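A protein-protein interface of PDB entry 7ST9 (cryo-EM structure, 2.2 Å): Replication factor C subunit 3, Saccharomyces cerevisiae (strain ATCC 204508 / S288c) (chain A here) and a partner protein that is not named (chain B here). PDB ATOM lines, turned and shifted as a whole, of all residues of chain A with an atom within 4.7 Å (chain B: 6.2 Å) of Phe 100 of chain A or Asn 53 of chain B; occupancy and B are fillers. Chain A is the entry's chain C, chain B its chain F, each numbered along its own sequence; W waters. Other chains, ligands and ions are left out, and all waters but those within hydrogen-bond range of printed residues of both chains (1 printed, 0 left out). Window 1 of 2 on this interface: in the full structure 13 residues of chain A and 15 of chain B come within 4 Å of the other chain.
Among the printed residues, pairs that only touch across the chains: Leu 80 of chain A with His 54 of chain B (3.8 Å), Gln 96 of chain A with Asn 53 of chain B (3.2 Å), Phe 100 of chain A with Asn 53 of chain B (3.9 Å) and Thr 103 of chain A with Val 55 of chain B (3.5 Å).
O of Leu 113 of chain A lies within hydrogen-bond range of N of Leu 80 of chain A (2.9 Å). The side-chain hydroxyl of Thr 103 of chain A sits at hydrogen-bond distance from the backbone carbonyl oxygen of Asp 99 of chain A (2.9 Å). O of Phe 100 of chain A sits at hydrogen-bond distance from OG1 of Thr 103 of chain A (2.9 Å). O of Phe 100 of chain A is in hydrogen-bond range of NZ of Lys 112 of chain A, at 2.7 Å. The side-chain amino group (NZ) of Lys 112 of chain A sits at hydrogen-bond distance from the side-chain hydroxyl (OG1) of Thr 103 of chain A, 2.7 Å away. OE1 of Glu 51 of chain B is in hydrogen-bond range of ND1 of His 54 of chain B (2.9 Å).
Of the printed residues of chain B, Leu 80 of chain A touches His 54. Printed residues of chain B within 4 Å of Gln 96 of chain A: Asn 53 (3.2 Å). Phe 100 of chain A touches just one residue of chain B: Asn 53 (3.9 Å). Of the printed residues of chain B, Thr 103 of chain A touches Val 55. Asn 53 of chain B touches two residues of chain A. Of the printed residues of chain A, His 54 of chain B touches Leu 80. Of the printed residues of chain A, Val 55 of chain B touches Thr 103 (3.5 Å). The nearest residue of chain B that does not touch Phe 100 of chain A is His 54 of chain B (4.1 Å).
Water W1 bridges NZ of Lys 112 of chain A (3.0 Å) and O of His 54 of chain B (3.2 Å).
Hydrophobic or aromatic side chains of chain A within 4 Å of the printed part of chain B: Leu 80 and Phe 100. Printed residues of chain B that touch a printed residue of chain A: Asn 53, His 54 and Val 55. Hydrophobic or aromatic side chains of chain B within 4 Å of the printed part of chain A: His 54 and Val 55. Among the printed residues, 4 pairs touch across the chains. Among the printed residues, no Asp or Glu carboxylate lies within 4 Å of a Lys or Arg side-chain nitrogen of the other chain.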
ATOM      1  N   MET A  78      -0.647 -24.313 -32.267  1.00  0.00           N
ATOM      2  CA  MET A  78      -1.062 -23.190 -31.433  1.00  0.00           C
ATOM      3  C   MET A  78      -2.298 -22.485 -31.983  1.00  0.00           C
ATOM      4  O   MET A  78      -2.559 -21.331 -31.629  1.00  0.00           O
ATOM      5  CB  MET A  78       0.085 -22.193 -31.275  1.00  0.00           C
ATOM      6  CG  MET A  78       0.832 -21.892 -32.565  1.00  0.00           C
ATOM      7  SD  MET A  78       2.127 -23.090 -32.943  1.00  0.00           S
ATOM      8  CE  MET A  78       3.187 -22.936 -31.505  1.00  0.00           C
ATOM      9  N   VAL A  79      -3.063 -23.153 -32.841  1.00  0.00           N
ATOM     10  CA  VAL A  79      -4.320 -22.631 -33.363  1.00  0.00           C
ATOM     11  C   VAL A  79      -5.417 -23.626 -33.019  1.00  0.00           C
ATOM     12  O   VAL A  79      -5.306 -24.814 -33.342  1.00  0.00           O
ATOM     13  CB  VAL A  79      -4.251 -22.392 -34.882  1.00  0.00           C
ATOM     14  CG1 VAL A  79      -5.625 -22.031 -35.430  1.00  0.00           C
ATOM     15  CG2 VAL A  79      -3.239 -21.303 -35.205  1.00  0.00           C
ATOM     16  N   LEU A  80      -6.471 -23.146 -32.361  1.00  0.00           N
ATOM     17  CA  LEU A  80      -7.624 -23.969 -32.010  1.00  0.00           C
ATOM     18  C   LEU A  80      -8.770 -23.598 -32.944  1.00  0.00           C
ATOM     19  O   LEU A  80      -9.345 -22.513 -32.827  1.00  0.00           O
ATOM     20  CB  LEU A  80      -8.020 -23.772 -30.547  1.00  0.00           C
ATOM     21  CG  LEU A  80      -9.324 -24.452 -30.114  1.00  0.00           C
ATOM     22  CD1 LEU A  80      -9.251 -25.957 -30.342  1.00  0.00           C
ATOM     23  CD2 LEU A  80      -9.641 -24.143 -28.659  1.00  0.00           C
ATOM     24  N   GLN A  96     -13.330 -26.480 -22.964  1.00  0.00           N
ATOM     25  CA  GLN A  96     -12.260 -26.632 -23.946  1.00  0.00           C
ATOM     26  C   GLN A  96     -11.689 -25.280 -24.357  1.00  0.00           C
ATOM     27  O   GLN A  96     -10.475 -25.052 -24.273  1.00  0.00           O
ATOM     28  CB  GLN A  96     -12.781 -27.393 -25.167  1.00  0.00           C
ATOM     29  CG  GLN A  96     -11.801 -27.460 -26.329  1.00  0.00           C
ATOM     30  CD  GLN A  96     -12.267 -28.389 -27.433  1.00  0.00           C
ATOM     31  OE1 GLN A  96     -13.417 -28.828 -27.446  1.00  0.00           O
ATOM     32  NE2 GLN A  96     -11.376 -28.689 -28.370  1.00  0.00           N
ATOM     33  N   ILE A  97     -12.555 -24.373 -24.813  1.00  0.00           N
ATOM     34  CA  ILE A  97     -12.092 -23.067 -25.267  1.00  0.00           C
ATOM     35  C   ILE A  97     -11.442 -22.309 -24.118  1.00  0.00           C
ATOM     36  O   ILE A  97     -10.391 -21.679 -24.287  1.00  0.00           O
ATOM     37  CB  ILE A  97     -13.261 -22.273 -25.884  1.00  0.00           C
ATOM     38  CG1 ILE A  97     -13.669 -22.895 -27.223  1.00  0.00           C
ATOM     39  CG2 ILE A  97     -12.879 -20.810 -26.064  1.00  0.00           C
ATOM     40  CD1 ILE A  97     -15.027 -22.451 -27.725  1.00  0.00           C
ATOM     41  N   LYS A  98     -12.052 -22.358 -22.934  1.00  0.00           N
ATOM     42  CA  LYS A  98     -11.503 -21.642 -21.789  1.00  0.00           C
ATOM     43  C   LYS A  98     -10.125 -22.177 -21.412  1.00  0.00           C
ATOM     44  O   LYS A  98      -9.194 -21.401 -21.170  1.00  0.00           O
ATOM     45  CB  LYS A  98     -12.462 -21.739 -20.603  1.00  0.00           C
ATOM     46  CG  LYS A  98     -12.178 -20.743 -19.493  1.00  0.00           C
ATOM     47  CD  LYS A  98     -13.264 -20.770 -18.431  1.00  0.00           C
ATOM     48  CE  LYS A  98     -12.850 -19.996 -17.191  1.00  0.00           C
ATOM     49  NZ  LYS A  98     -13.923 -19.079 -16.718  1.00  0.00           N
ATOM     50  N   ASP A  99      -9.971 -23.505 -21.360  1.00  0.00           N
ATOM     51  CA  ASP A  99      -8.677 -24.075 -21.000  1.00  0.00           C
ATOM     52  C   ASP A  99      -7.619 -23.746 -22.043  1.00  0.00           C
ATOM     53  O   ASP A  99      -6.472 -23.439 -21.697  1.00  0.00           O
ATOM     54  CB  ASP A  99      -8.799 -25.588 -20.813  1.00  0.00           C
ATOM     55  CG  ASP A  99      -9.777 -25.964 -19.714  1.00  0.00           C
ATOM     56  OD1 ASP A  99      -9.855 -25.228 -18.707  1.00  0.00           O
ATOM     57  OD2 ASP A  99     -10.463 -26.999 -19.852  1.00  0.00           O
ATOM     58  N   PHE A 100      -7.974 -23.809 -23.329  1.00  0.00           N
ATOM     59  CA  PHE A 100      -7.002 -23.463 -24.363  1.00  0.00           C
ATOM     60  C   PHE A 100      -6.599 -21.996 -24.272  1.00  0.00           C
ATOM     61  O   PHE A 100      -5.420 -21.658 -24.422  1.00  0.00           O
ATOM     62  CB  PHE A 100      -7.564 -23.774 -25.749  1.00  0.00           C
ATOM     63  CG  PHE A 100      -6.614 -23.448 -26.868  1.00  0.00           C
ATOM     64  CD1 PHE A 100      -5.613 -24.334 -27.224  1.00  0.00           C
ATOM     65  CD2 PHE A 100      -6.718 -22.251 -27.555  1.00  0.00           C
ATOM     66  CE1 PHE A 100      -4.737 -24.037 -28.251  1.00  0.00           C
ATOM     67  CE2 PHE A 100      -5.844 -21.947 -28.583  1.00  0.00           C
ATOM     68  CZ  PHE A 100      -4.852 -22.841 -28.931  1.00  0.00           C
ATOM     69  N   ALA A 101      -7.565 -21.108 -24.026  1.00  0.00           N
ATOM     70  CA  ALA A 101      -7.273 -19.680 -23.991  1.00  0.00           C
ATOM     71  C   ALA A 101      -6.511 -19.268 -22.739  1.00  0.00           C
ATOM     72  O   ALA A 101      -5.848 -18.225 -22.751  1.00  0.00           O
ATOM     73  CB  ALA A 101      -8.569 -18.876 -24.091  1.00  0.00           C
ATOM     74  N   SER A 102      -6.585 -20.055 -21.668  1.00  0.00           N
ATOM     75  CA  SER A 102      -5.965 -19.711 -20.396  1.00  0.00           C
ATOM     76  C   SER A 102      -4.638 -20.428 -20.169  1.00  0.00           C
ATOM     77  O   SER A 102      -4.091 -20.357 -19.064  1.00  0.00           O
ATOM     78  CB  SER A 102      -6.925 -20.024 -19.247  1.00  0.00           C
ATOM     79  OG  SER A 102      -7.145 -21.418 -19.129  1.00  0.00           O
ATOM     80  N   THR A 103      -4.109 -21.110 -21.179  1.00  0.00           N
ATOM     81  CA  THR A 103      -2.848 -21.828 -21.070  1.00  0.00           C
ATOM     82  C   THR A 103      -1.770 -21.121 -21.881  1.00  0.00           C
ATOM     83  O   THR A 103      -2.054 -20.394 -22.837  1.00  0.00           O
ATOM     84  CB  THR A 103      -2.992 -23.279 -21.547  1.00  0.00           C
ATOM     85  OG1 THR A 103      -3.803 -23.327 -22.727  1.00  0.00           O
ATOM     86  CG2 THR A 103      -3.619 -24.142 -20.461  1.00  0.00           C
ATOM     87  N   LYS A 112      -1.834 -16.996 -28.671  1.00  0.00           N
ATOM     88  CA  LYS A 112      -2.560 -18.100 -29.278  1.00  0.00           C
ATOM     89  C   LYS A 112      -3.743 -17.572 -30.084  1.00  0.00           C
ATOM     90  O   LYS A 112      -4.211 -16.448 -29.885  1.00  0.00           O
ATOM     91  CB  LYS A 112      -3.046 -19.077 -28.206  1.00  0.00           C
ATOM     92  CG  LYS A 112      -1.997 -19.422 -27.158  1.00  0.00           C
ATOM     93  CD  LYS A 112      -2.578 -20.268 -26.038  1.00  0.00           C
ATOM     94  CE  LYS A 112      -2.478 -21.750 -26.352  1.00  0.00           C
ATOM     95  NZ  LYS A 112      -2.994 -22.596 -25.242  1.00  0.00           N
ATOM     96  N   LEU A 113      -4.226 -18.404 -31.004  1.00  0.00           N
ATOM     97  CA  LEU A 113      -5.314 -18.039 -31.900  1.00  0.00           C
ATOM     98  C   LEU A 113      -6.439 -19.059 -31.789  1.00  0.00           C
ATOM     99  O   LEU A 113      -6.196 -20.271 -31.845  1.00  0.00           O
ATOM    100  CB  LEU A 113      -4.821 -17.949 -33.349  1.00  0.00           C
ATOM    101  CG  LEU A 113      -5.854 -17.518 -34.393  1.00  0.00           C
ATOM    102  CD1 LEU A 113      -6.350 -16.108 -34.116  1.00  0.00           C
ATOM    103  CD2 LEU A 113      -5.271 -17.615 -35.793  1.00  0.00           C
ATOM    104  N   ILE A 114      -7.662 -18.561 -31.627  1.00  0.00           N
ATOM    105  CA  ILE A 114      -8.866 -19.384 -31.623  1.00  0.00           C
ATOM    106  C   ILE A 114      -9.734 -18.932 -32.788  1.00  0.00           C
ATOM    107  O   ILE A 114     -10.103 -17.754 -32.875  1.00  0.00           O
ATOM    108  CB  ILE A 114      -9.632 -19.281 -30.295  1.00  0.00           C
ATOM    109  CG1 ILE A 114      -8.827 -19.932 -29.169  1.00  0.00           C
ATOM    110  CG2 ILE A 114     -11.004 -19.936 -30.423  1.00  0.00           C
ATOM    111  CD1 ILE A 114      -9.330 -19.600 -27.783  1.00  0.00           C
ATOM    112  N   GLU B  51      -4.080 -37.011 -26.658  1.00  0.00           N
ATOM    113  CA  GLU B  51      -3.957 -35.592 -26.363  1.00  0.00           C
ATOM    114  C   GLU B  51      -5.327 -35.034 -26.016  1.00  0.00           C
ATOM    115  O   GLU B  51      -6.339 -35.457 -26.582  1.00  0.00           O
ATOM    116  CB  GLU B  51      -3.357 -34.820 -27.548  1.00  0.00           C
ATOM    117  CG  GLU B  51      -4.318 -34.601 -28.710  1.00  0.00           C
ATOM    118  CD  GLU B  51      -5.103 -33.307 -28.585  1.00  0.00           C
ATOM    119  OE1 GLU B  51      -4.476 -32.227 -28.562  1.00  0.00           O
ATOM    120  OE2 GLU B  51      -6.349 -33.370 -28.507  1.00  0.00           O
ATOM    121  N   ASN B  52      -5.353 -34.089 -25.080  1.00  0.00           N
ATOM    122  CA  ASN B  52      -6.578 -33.421 -24.662  1.00  0.00           C
ATOM    123  C   ASN B  52      -6.408 -31.913 -24.781  1.00  0.00           C
ATOM    124  O   ASN B  52      -5.448 -31.340 -24.240  1.00  0.00           O
ATOM    125  CB  ASN B  52      -6.965 -33.797 -23.225  1.00  0.00           C
ATOM    126  CG  ASN B  52      -7.891 -35.006 -23.150  1.00  0.00           C
ATOM    127  OD1 ASN B  52      -8.667 -35.137 -22.204  1.00  0.00           O
ATOM    128  ND2 ASN B  52      -7.811 -35.894 -24.136  1.00  0.00           N
ATOM    129  N   ASN B  53      -7.339 -31.295 -25.514  1.00  0.00           N
ATOM    130  CA  ASN B  53      -7.519 -29.844 -25.596  1.00  0.00           C
ATOM    131  C   ASN B  53      -6.247 -29.122 -26.020  1.00  0.00           C
ATOM    132  O   ASN B  53      -6.083 -27.930 -25.748  1.00  0.00           O
ATOM    133  CB  ASN B  53      -8.035 -29.285 -24.266  1.00  0.00           C
ATOM    134  CG  ASN B  53      -9.464 -29.701 -23.974  1.00  0.00           C
ATOM    135  OD1 ASN B  53     -10.259 -29.919 -24.889  1.00  0.00           O
ATOM    136  ND2 ASN B  53      -9.799 -29.817 -22.695  1.00  0.00           N
ATOM    137  N   HIS B  54      -5.340 -29.820 -26.700  1.00  0.00           N
ATOM    138  CA  HIS B  54      -4.036 -29.291 -27.084  1.00  0.00           C
ATOM    139  C   HIS B  54      -3.227 -28.818 -25.885  1.00  0.00           C
ATOM    140  O   HIS B  54      -2.208 -28.138 -26.062  1.00  0.00           O
ATOM    141  CB  HIS B  54      -4.173 -28.144 -28.094  1.00  0.00           C
ATOM    142  CG  HIS B  54      -5.005 -28.485 -29.291  1.00  0.00           C
ATOM    143  ND1 HIS B  54      -4.913 -29.698 -29.940  1.00  0.00           N
ATOM    144  CD2 HIS B  54      -5.942 -27.773 -29.958  1.00  0.00           C
ATOM    145  CE1 HIS B  54      -5.759 -29.718 -30.954  1.00  0.00           C
ATOM    146  NE2 HIS B  54      -6.396 -28.561 -30.987  1.00  0.00           N
ATOM    147  N   VAL B  55      -3.647 -29.163 -24.668  1.00  0.00           N
ATOM    148  CA  VAL B  55      -2.965 -28.718 -23.467  1.00  0.00           C
ATOM    149  C   VAL B  55      -2.274 -29.861 -22.733  1.00  0.00           C
ATOM    150  O   VAL B  55      -1.294 -29.612 -22.021  1.00  0.00           O
ATOM    151  CB  VAL B  55      -3.929 -27.973 -22.518  1.00  0.00           C
ATOM    152  CG1 VAL B  55      -4.441 -26.694 -23.167  1.00  0.00           C
ATOM    153  CG2 VAL B  55      -5.077 -28.875 -22.092  1.00  0.00           C
ATOM    154  N   ILE B  56      -2.747 -31.102 -22.870  1.00  0.00           N
ATOM    155  CA  ILE B  56      -2.086 -32.220 -22.206  1.00  0.00           C
ATOM    156  C   ILE B  56      -1.914 -33.374 -23.183  1.00  0.00           C
ATOM    157  O   ILE B  56      -2.699 -33.545 -24.120  1.00  0.00           O
ATOM    158  CB  ILE B  56      -2.852 -32.671 -20.942  1.00  0.00           C
ATOM    159  CG1 ILE B  56      -2.039 -33.712 -20.168  1.00  0.00           C
ATOM    160  CG2 ILE B  56      -4.212 -33.219 -21.301  1.00  0.00           C
ATOM    161  CD1 ILE B  56      -2.451 -33.849 -18.719  1.00  0.00           C
ATOM    162  N   LYS B 244      -5.105 -36.133 -14.331  1.00  0.00           N
ATOM    163  CA  LYS B 244      -5.128 -37.187 -15.335  1.00  0.00           C
ATOM    164  C   LYS B 244      -3.961 -38.157 -15.204  1.00  0.00           C
ATOM    165  O   LYS B 244      -3.961 -39.190 -15.883  1.00  0.00           O
ATOM    166  CB  LYS B 244      -5.140 -36.571 -16.736  1.00  0.00           C
ATOM    167  CG  LYS B 244      -6.516 -36.092 -17.169  1.00  0.00           C
ATOM    168  CD  LYS B 244      -6.453 -35.205 -18.398  1.00  0.00           C
ATOM    169  CE  LYS B 244      -7.837 -34.704 -18.784  1.00  0.00           C
ATOM    170  NZ  LYS B 244      -7.784 -33.671 -19.854  1.00  0.00           N
HETATM  171  O   HOH W   1      -1.804 -25.016 -26.528  1.00  0.00           O
